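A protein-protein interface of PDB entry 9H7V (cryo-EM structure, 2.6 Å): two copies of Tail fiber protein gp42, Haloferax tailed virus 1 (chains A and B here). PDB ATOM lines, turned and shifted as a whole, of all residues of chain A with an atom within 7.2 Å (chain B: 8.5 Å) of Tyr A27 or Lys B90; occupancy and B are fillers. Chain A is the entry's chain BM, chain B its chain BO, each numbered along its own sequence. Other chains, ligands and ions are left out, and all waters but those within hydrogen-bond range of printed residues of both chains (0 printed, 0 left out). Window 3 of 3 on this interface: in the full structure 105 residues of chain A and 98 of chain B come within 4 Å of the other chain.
The side-chain amide oxygen (OE1) of Gln B85 lies within hydrogen-bond range of the side-chain hydroxyl (OG) of Ser A29 (2.5 Å). The backbone NH (N) of Ala A30 lies within hydrogen-bond range of the side-chain carboxylate (OD2) of Asp B15 (2.7 Å). OH of Tyr A32 lies within hydrogen-bond range of O of Gln B85.
The backbone carbonyl oxygen (O) of Val B84 lies within hydrogen-bond range of the backbone NH (N) of Asp B93 (3.0 Å). The side-chain hydroxyl (OH) of Tyr B92 is in hydrogen-bond range of the side-chain carboxylate (OD2) of Asp B15 (2.7 Å). O of Asp A24 is in hydrogen-bond range of ND2 of Asn A132, at 2.8 Å. The side-chain amide nitrogen (NE2) of Gln B85 lies within hydrogen-bond range of the backbone carbonyl oxygen (O) of Lys B90.
Among the printed residues, merely in contact across the chains: Asp A24 with Ser B88 (3.5 Å), Asp A26 with Gly B87 (3.8 Å), Tyr A27 with Gln B85 (3.6 Å), Tyr A27 with Gly B87 (3.7 Å), Tyr A27 with Ser B88 (3.3 Å), Tyr A27 with Gln B89 (3.1 Å), Tyr A27 with Lys B90 (3.9 Å), Ser A29 with Asp B15 (3.5 Å), Tyr A32 with Val B84 (3.7 Å) and Asn A132 with Gly B87 (3.6 Å).
Of the printed residues of chain B, Asp A26 touches Gly B87 (3.8 Å). Of chain B, only Gln B85, Gly B87, Ser B88, Gln B89 and Lys B90 come within 4 Å of Tyr A27. Of the printed residues of chain B, Ala A30 touches Asp B15 (2.7 Å). Of the printed residues of chain B, Asn A132 touches Gly B87 (3.6 Å). Of the printed residues of chain A, Asp B15 touches Ser A29 and Ala A30. Of the printed residues of chain A, Gln B89 touches Tyr A27 (3.1 Å). Lys B90 touches just one residue of chain A: Tyr A27. The nearest residue of chain B that does not touch Tyr A27 is Ser B86 (6.1 Å). The nearest residue of chain A that does not touch Lys B90 is Ser A29 (6.8 Å).
Hydrophobic or aromatic side chains of chain B within 4 Å of the printed part of chain A: Val B84. Hydrophobic or aromatic side chains of chain A that line the printed part of chain B: Tyr A27, Ala A30 and Tyr A32. Among the printed residues, no Asp or Glu carboxylate lies within 4 Å of a Lys or Arg side-chain nitrogen of the other chain.
Position printed for both chains: 25. Of the 13 pairs that touch across the chains among the printed residues, none has its exchanged pair printed and touching as well.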
ATOM      1  N   PHE A  12     -14.679  10.542 -30.819  1.00  0.00           N
ATOM      2  CA  PHE A  12     -13.799   9.732 -29.986  1.00  0.00           C
ATOM      3  C   PHE A  12     -12.344  10.018 -30.360  1.00  0.00           C
ATOM      4  O   PHE A  12     -12.069  10.253 -31.536  1.00  0.00           O
ATOM      5  CB  PHE A  12     -14.120   8.246 -30.186  1.00  0.00           C
ATOM      6  CG  PHE A  12     -13.283   7.281 -29.383  1.00  0.00           C
ATOM      7  CD1 PHE A  12     -13.634   6.951 -28.080  1.00  0.00           C
ATOM      8  CD2 PHE A  12     -12.139   6.705 -29.925  1.00  0.00           C
ATOM      9  CE1 PHE A  12     -12.862   6.065 -27.338  1.00  0.00           C
ATOM     10  CE2 PHE A  12     -11.367   5.821 -29.181  1.00  0.00           C
ATOM     11  CZ  PHE A  12     -11.731   5.503 -27.889  1.00  0.00           C
ATOM     12  N   PRO A  13     -11.351   9.993 -29.429  1.00  0.00           N
ATOM     13  CA  PRO A  13     -11.565   9.871 -27.980  1.00  0.00           C
ATOM     14  C   PRO A  13     -11.557  11.197 -27.213  1.00  0.00           C
ATOM     15  O   PRO A  13     -10.965  12.171 -27.675  1.00  0.00           O
ATOM     16  CB  PRO A  13     -10.357   8.998 -27.600  1.00  0.00           C
ATOM     17  CG  PRO A  13      -9.243   9.411 -28.548  1.00  0.00           C
ATOM     18  CD  PRO A  13      -9.919   9.997 -29.769  1.00  0.00           C
ATOM     19  N   GLN A  14     -12.207  11.228 -26.034  1.00  0.00           N
ATOM     20  CA  GLN A  14     -12.388  12.462 -25.271  1.00  0.00           C
ATOM     21  C   GLN A  14     -12.142  12.245 -23.773  1.00  0.00           C
ATOM     22  O   GLN A  14     -12.656  11.291 -23.189  1.00  0.00           O
ATOM     23  CB  GLN A  14     -13.767  13.075 -25.538  1.00  0.00           C
ATOM     24  CG  GLN A  14     -13.961  13.588 -26.961  1.00  0.00           C
ATOM     25  CD  GLN A  14     -15.365  14.072 -27.227  1.00  0.00           C
ATOM     26  OE1 GLN A  14     -16.264  13.296 -27.548  1.00  0.00           O
ATOM     27  NE2 GLN A  14     -15.562  15.375 -27.104  1.00  0.00           N
ATOM     28  N   GLY A  23     -17.140  14.192 -15.453  1.00  0.00           N
ATOM     29  CA  GLY A  23     -18.101  13.103 -15.545  1.00  0.00           C
ATOM     30  C   GLY A  23     -18.301  12.596 -16.974  1.00  0.00           C
ATOM     31  O   GLY A  23     -18.953  11.571 -17.172  1.00  0.00           O
ATOM     32  N   ASP A  24     -17.709  13.296 -17.955  1.00  0.00           N
ATOM     33  CA  ASP A  24     -18.180  13.253 -19.334  1.00  0.00           C
ATOM     34  C   ASP A  24     -17.141  12.688 -20.307  1.00  0.00           C
ATOM     35  O   ASP A  24     -17.260  12.910 -21.512  1.00  0.00           O
ATOM     36  CB  ASP A  24     -18.627  14.641 -19.809  1.00  0.00           C
ATOM     37  CG  ASP A  24     -19.632  15.342 -18.908  1.00  0.00           C
ATOM     38  OD1 ASP A  24     -20.525  14.657 -18.366  1.00  0.00           O
ATOM     39  OD2 ASP A  24     -19.519  16.575 -18.765  1.00  0.00           O
ATOM     40  N   GLU A  25     -16.144  11.949 -19.802  1.00  0.00           N
ATOM     41  CA  GLU A  25     -15.141  11.318 -20.650  1.00  0.00           C
ATOM     42  C   GLU A  25     -15.789  10.168 -21.424  1.00  0.00           C
ATOM     43  O   GLU A  25     -16.714   9.536 -20.918  1.00  0.00           O
ATOM     44  CB  GLU A  25     -13.943  10.871 -19.805  1.00  0.00           C
ATOM     45  CG  GLU A  25     -13.259  12.021 -19.080  1.00  0.00           C
ATOM     46  CD  GLU A  25     -12.062  11.658 -18.219  1.00  0.00           C
ATOM     47  OE1 GLU A  25     -12.270  11.133 -17.106  1.00  0.00           O
ATOM     48  OE2 GLU A  25     -10.922  11.907 -18.659  1.00  0.00           O
ATOM     49  N   ASP A  26     -15.306   9.916 -22.653  1.00  0.00           N
ATOM     50  CA  ASP A  26     -15.854   8.898 -23.542  1.00  0.00           C
ATOM     51  C   ASP A  26     -15.726   7.510 -22.914  1.00  0.00           C
ATOM     52  O   ASP A  26     -14.877   7.290 -22.051  1.00  0.00           O
ATOM     53  CB  ASP A  26     -15.129   8.867 -24.892  1.00  0.00           C
ATOM     54  CG  ASP A  26     -15.642   9.825 -25.956  1.00  0.00           C
ATOM     55  OD1 ASP A  26     -16.863  10.098 -25.989  1.00  0.00           O
ATOM     56  OD2 ASP A  26     -14.809  10.273 -26.765  1.00  0.00           O
ATOM     57  N   TYR A  27     -16.572   6.580 -23.378  1.00  0.00           N
ATOM     58  CA  TYR A  27     -16.476   5.179 -23.000  1.00  0.00           C
ATOM     59  C   TYR A  27     -15.595   4.413 -23.986  1.00  0.00           C
ATOM     60  O   TYR A  27     -15.467   4.784 -25.152  1.00  0.00           O
ATOM     61  CB  TYR A  27     -17.856   4.547 -22.791  1.00  0.00           C
ATOM     62  CG  TYR A  27     -18.291   4.454 -21.349  1.00  0.00           C
ATOM     63  CD1 TYR A  27     -18.960   5.504 -20.737  1.00  0.00           C
ATOM     64  CD2 TYR A  27     -18.036   3.318 -20.592  1.00  0.00           C
ATOM     65  CE1 TYR A  27     -19.375   5.426 -19.416  1.00  0.00           C
ATOM     66  CE2 TYR A  27     -18.436   3.227 -19.267  1.00  0.00           C
ATOM     67  CZ  TYR A  27     -19.105   4.286 -18.676  1.00  0.00           C
ATOM     68  OH  TYR A  27     -19.504   4.208 -17.374  1.00  0.00           O
ATOM     69  N   ASP A  28     -15.045   3.307 -23.471  1.00  0.00           N
ATOM     70  CA  ASP A  28     -13.903   2.563 -23.973  1.00  0.00           C
ATOM     71  C   ASP A  28     -14.398   1.431 -24.879  1.00  0.00           C
ATOM     72  O   ASP A  28     -14.171   0.258 -24.587  1.00  0.00           O
ATOM     73  CB  ASP A  28     -13.097   2.110 -22.743  1.00  0.00           C
ATOM     74  CG  ASP A  28     -12.005   1.072 -22.946  1.00  0.00           C
ATOM     75  OD1 ASP A  28     -11.293   1.151 -23.966  1.00  0.00           O
ATOM     76  OD2 ASP A  28     -11.870   0.192 -22.068  1.00  0.00           O
ATOM     77  N   SER A  29     -15.078   1.775 -25.985  1.00  0.00           N
ATOM     78  CA  SER A  29     -15.686   0.769 -26.849  1.00  0.00           C
ATOM     79  C   SER A  29     -14.644   0.137 -27.770  1.00  0.00           C
ATOM     80  O   SER A  29     -13.662   0.782 -28.132  1.00  0.00           O
ATOM     81  CB  SER A  29     -16.840   1.330 -27.646  1.00  0.00           C
ATOM     82  OG  SER A  29     -17.731   2.065 -26.823  1.00  0.00           O
ATOM     83  N   ALA A  30     -14.885  -1.130 -28.144  1.00  0.00           N
ATOM     84  CA  ALA A  30     -14.051  -1.865 -29.084  1.00  0.00           C
ATOM     85  C   ALA A  30     -14.107  -1.207 -30.460  1.00  0.00           C
ATOM     86  O   ALA A  30     -13.067  -0.980 -31.076  1.00  0.00           O
ATOM     87  CB  ALA A  30     -14.476  -3.313 -29.147  1.00  0.00           C
ATOM     88  N   TYR A  32     -14.753   1.813 -31.270  1.00  0.00           N
ATOM     89  CA  TYR A  32     -14.069   3.097 -31.238  1.00  0.00           C
ATOM     90  C   TYR A  32     -12.566   2.909 -31.435  1.00  0.00           C
ATOM     91  O   TYR A  32     -11.946   3.693 -32.151  1.00  0.00           O
ATOM     92  CB  TYR A  32     -14.321   3.828 -29.917  1.00  0.00           C
ATOM     93  CG  TYR A  32     -15.614   4.595 -29.773  1.00  0.00           C
ATOM     94  CD1 TYR A  32     -16.187   5.297 -30.828  1.00  0.00           C
ATOM     95  CD2 TYR A  32     -16.236   4.667 -28.536  1.00  0.00           C
ATOM     96  CE1 TYR A  32     -17.366   6.012 -30.661  1.00  0.00           C
ATOM     97  CE2 TYR A  32     -17.411   5.378 -28.351  1.00  0.00           C
ATOM     98  CZ  TYR A  32     -17.979   6.054 -29.419  1.00  0.00           C
ATOM     99  OH  TYR A  32     -19.136   6.757 -29.248  1.00  0.00           O
ATOM    100  N   ASN A 132     -19.405  16.210 -24.739  1.00  0.00           N
ATOM    101  CA  ASN A 132     -19.182  14.931 -25.395  1.00  0.00           C
ATOM    102  C   ASN A 132     -20.128  14.775 -26.586  1.00  0.00           C
ATOM    103  O   ASN A 132     -21.341  14.915 -26.439  1.00  0.00           O
ATOM    104  CB  ASN A 132     -19.259  13.759 -24.410  1.00  0.00           C
ATOM    105  CG  ASN A 132     -18.527  12.523 -24.893  1.00  0.00           C
ATOM    106  OD1 ASN A 132     -18.478  12.241 -26.088  1.00  0.00           O
ATOM    107  ND2 ASN A 132     -17.960  11.770 -23.966  1.00  0.00           N
ATOM    108  N   ASP B  15     -15.807  -6.481 -27.476  1.00  0.00           N
ATOM    109  CA  ASP B  15     -16.748  -6.244 -26.389  1.00  0.00           C
ATOM    110  C   ASP B  15     -18.143  -6.592 -26.908  1.00  0.00           C
ATOM    111  O   ASP B  15     -18.269  -7.014 -28.053  1.00  0.00           O
ATOM    112  CB  ASP B  15     -16.637  -4.814 -25.850  1.00  0.00           C
ATOM    113  CG  ASP B  15     -16.954  -3.719 -26.859  1.00  0.00           C
ATOM    114  OD1 ASP B  15     -17.522  -4.024 -27.928  1.00  0.00           O
ATOM    115  OD2 ASP B  15     -16.626  -2.554 -26.563  1.00  0.00           O
ATOM    116  N   ASP B  16     -19.190  -6.395 -26.095  1.00  0.00           N
ATOM    117  CA  ASP B  16     -20.529  -6.817 -26.491  1.00  0.00           C
ATOM    118  C   ASP B  16     -21.110  -5.912 -27.581  1.00  0.00           C
ATOM    119  O   ASP B  16     -22.207  -6.175 -28.073  1.00  0.00           O
ATOM    120  CB  ASP B  16     -21.460  -7.008 -25.291  1.00  0.00           C
ATOM    121  CG  ASP B  16     -21.508  -5.795 -24.386  1.00  0.00           C
ATOM    122  OD1 ASP B  16     -22.424  -4.974 -24.562  1.00  0.00           O
ATOM    123  OD2 ASP B  16     -20.621  -5.683 -23.523  1.00  0.00           O
ATOM    124  N   ASN B  22     -21.609 -10.592 -22.324  1.00  0.00           N
ATOM    125  CA  ASN B  22     -21.232  -9.497 -21.436  1.00  0.00           C
ATOM    126  C   ASN B  22     -20.078  -9.886 -20.510  1.00  0.00           C
ATOM    127  O   ASN B  22     -19.350  -9.014 -20.036  1.00  0.00           O
ATOM    128  CB  ASN B  22     -22.430  -8.909 -20.680  1.00  0.00           C
ATOM    129  CG  ASN B  22     -22.116  -7.609 -19.965  1.00  0.00           C
ATOM    130  OD1 ASN B  22     -21.469  -6.722 -20.518  1.00  0.00           O
ATOM    131  ND2 ASN B  22     -22.574  -7.485 -18.730  1.00  0.00           N
ATOM    132  N   GLU B  25     -15.745  -9.929 -22.564  1.00  0.00           N
ATOM    133  CA  GLU B  25     -15.075  -8.771 -23.144  1.00  0.00           C
ATOM    134  C   GLU B  25     -13.557  -8.964 -23.075  1.00  0.00           C
ATOM    135  O   GLU B  25     -13.067  -9.692 -22.213  1.00  0.00           O
ATOM    136  CB  GLU B  25     -15.485  -7.493 -22.407  1.00  0.00           C
ATOM    137  CG  GLU B  25     -16.985  -7.238 -22.389  1.00  0.00           C
ATOM    138  CD  GLU B  25     -17.494  -6.474 -21.177  1.00  0.00           C
ATOM    139  OE1 GLU B  25     -17.007  -6.737 -20.058  1.00  0.00           O
ATOM    140  OE2 GLU B  25     -18.378  -5.616 -21.354  1.00  0.00           O
ATOM    141  N   VAL B  84     -21.326   0.845 -30.756  1.00  0.00           N
ATOM    142  CA  VAL B  84     -20.475   1.596 -29.840  1.00  0.00           C
ATOM    143  C   VAL B  84     -21.350   2.373 -28.854  1.00  0.00           C
ATOM    144  O   VAL B  84     -22.567   2.450 -29.024  1.00  0.00           O
ATOM    145  CB  VAL B  84     -19.460   2.505 -30.568  1.00  0.00           C
ATOM    146  CG1 VAL B  84     -18.435   1.715 -31.366  1.00  0.00           C
ATOM    147  CG2 VAL B  84     -20.121   3.566 -31.438  1.00  0.00           C
ATOM    148  N   GLN B  85     -20.708   2.952 -27.831  1.00  0.00           N
ATOM    149  CA  GLN B  85     -21.380   3.643 -26.740  1.00  0.00           C
ATOM    150  C   GLN B  85     -21.357   5.148 -27.004  1.00  0.00           C
ATOM    151  O   GLN B  85     -20.285   5.746 -27.066  1.00  0.00           O
ATOM    152  CB  GLN B  85     -20.696   3.306 -25.410  1.00  0.00           C
ATOM    153  CG  GLN B  85     -20.753   1.829 -25.031  1.00  0.00           C
ATOM    154  CD  GLN B  85     -19.620   1.391 -24.131  1.00  0.00           C
ATOM    155  OE1 GLN B  85     -18.452   1.401 -24.513  1.00  0.00           O
ATOM    156  NE2 GLN B  85     -19.962   0.983 -22.921  1.00  0.00           N
ATOM    157  N   SER B  86     -22.547   5.750 -27.152  1.00  0.00           N
ATOM    158  CA  SER B  86     -22.675   7.185 -27.375  1.00  0.00           C
ATOM    159  C   SER B  86     -22.281   7.955 -26.117  1.00  0.00           C
ATOM    160  O   SER B  86     -22.734   7.628 -25.023  1.00  0.00           O
ATOM    161  CB  SER B  86     -24.067   7.554 -27.823  1.00  0.00           C
ATOM    162  OG  SER B  86     -24.186   8.958 -28.009  1.00  0.00           O
ATOM    163  N   GLY B  87     -21.418   8.964 -26.299  1.00  0.00           N
ATOM    164  CA  GLY B  87     -21.063   9.942 -25.280  1.00  0.00           C
ATOM    165  C   GLY B  87     -20.604   9.315 -23.965  1.00  0.00           C
ATOM    166  O   GLY B  87     -19.656   8.532 -23.938  1.00  0.00           O
ATOM    167  N   SER B  88     -21.317   9.672 -22.888  1.00  0.00           N
ATOM    168  CA  SER B  88     -20.991   9.294 -21.521  1.00  0.00           C
ATOM    169  C   SER B  88     -21.753   8.038 -21.093  1.00  0.00           C
ATOM    170  O   SER B  88     -21.696   7.659 -19.923  1.00  0.00           O
ATOM    171  CB  SER B  88     -21.272  10.439 -20.572  1.00  0.00           C
ATOM    172  OG  SER B  88     -20.720  11.657 -21.050  1.00  0.00           O
ATOM    173  N   GLN B  89     -22.453   7.388 -22.033  1.00  0.00           N
ATOM    174  CA  GLN B  89     -23.379   6.314 -21.700  1.00  0.00           C
ATOM    175  C   GLN B  89     -22.644   4.992 -21.499  1.00  0.00           C
ATOM    176  O   GLN B  89     -21.646   4.720 -22.165  1.00  0.00           O
ATOM    177  CB  GLN B  89     -24.439   6.119 -22.790  1.00  0.00           C
ATOM    178  CG  GLN B  89     -25.342   7.325 -23.020  1.00  0.00           C
ATOM    179  CD  GLN B  89     -26.238   7.675 -21.855  1.00  0.00           C
ATOM    180  OE1 GLN B  89     -26.488   6.872 -20.958  1.00  0.00           O
ATOM    181  NE2 GLN B  89     -26.751   8.895 -21.872  1.00  0.00           N
ATOM    182  N   LYS B  90     -23.186   4.168 -20.590  1.00  0.00           N
ATOM    183  CA  LYS B  90     -22.821   2.768 -20.448  1.00  0.00           C
ATOM    184  C   LYS B  90     -23.269   1.982 -21.679  1.00  0.00           C
ATOM    185  O   LYS B  90     -22.546   1.099 -22.136  1.00  0.00           O
ATOM    186  CB  LYS B  90     -23.529   2.140 -19.243  1.00  0.00           C
ATOM    187  CG  LYS B  90     -22.967   2.458 -17.866  1.00  0.00           C
ATOM    188  CD  LYS B  90     -23.657   1.641 -16.795  1.00  0.00           C
ATOM    189  CE  LYS B  90     -23.222   1.992 -15.388  1.00  0.00           C
ATOM    190  NZ  LYS B  90     -23.921   1.162 -14.379  1.00  0.00           N
ATOM    191  N   THR B  91     -24.463   2.301 -22.200  1.00  0.00           N
ATOM    192  CA  THR B  91     -25.159   1.439 -23.148  1.00  0.00           C
ATOM    193  C   THR B  91     -24.552   1.542 -24.544  1.00  0.00           C
ATOM    194  O   THR B  91     -24.248   2.636 -25.018  1.00  0.00           O
ATOM    195  CB  THR B  91     -26.661   1.746 -23.229  1.00  0.00           C
ATOM    196  OG1 THR B  91     -26.850   3.124 -23.558  1.00  0.00           O
ATOM    197  CG2 THR B  91     -27.417   1.400 -21.965  1.00  0.00           C
ATOM    198  N   TYR B  92     -24.402   0.380 -25.192  1.00  0.00           N
ATOM    199  CA  TYR B  92     -24.084   0.300 -26.608  1.00  0.00           C
ATOM    200  C   TYR B  92     -25.352   0.611 -27.398  1.00  0.00           C
ATOM    201  O   TYR B  92     -26.341  -0.114 -27.289  1.00  0.00           O
ATOM    202  CB  TYR B  92     -23.526  -1.082 -26.957  1.00  0.00           C
ATOM    203  CG  TYR B  92     -22.184  -1.395 -26.347  1.00  0.00           C
ATOM    204  CD1 TYR B  92     -22.075  -1.781 -25.018  1.00  0.00           C
ATOM    205  CD2 TYR B  92     -21.019  -1.305 -27.096  1.00  0.00           C
ATOM    206  CE1 TYR B  92     -20.846  -2.069 -24.448  1.00  0.00           C
ATOM    207  CE2 TYR B  92     -19.781  -1.596 -26.541  1.00  0.00           C
ATOM    208  CZ  TYR B  92     -19.696  -1.978 -25.213  1.00  0.00           C
ATOM    209  OH  TYR B  92     -18.490  -2.263 -24.645  1.00  0.00           O
ATOM    210  N   ASP B  93     -25.303   1.688 -28.195  1.00  0.00           N
ATOM    211  CA  ASP B  93     -26.502   2.263 -28.790  1.00  0.00           C
ATOM    212  C   ASP B  93     -26.284   2.689 -30.244  1.00  0.00           C
ATOM    213  O   ASP B  93     -27.251   2.783 -30.999  1.00  0.00           O
ATOM    214  CB  ASP B  93     -27.043   3.417 -27.938  1.00  0.00           C
ATOM    215  CG  ASP B  93     -25.995   4.450 -27.556  1.00  0.00           C
ATOM    216  OD1 ASP B  93     -25.126   4.749 -28.398  1.00  0.00           O
ATOM    217  OD2 ASP B  93     -26.047   4.938 -26.412  1.00  0.00           O
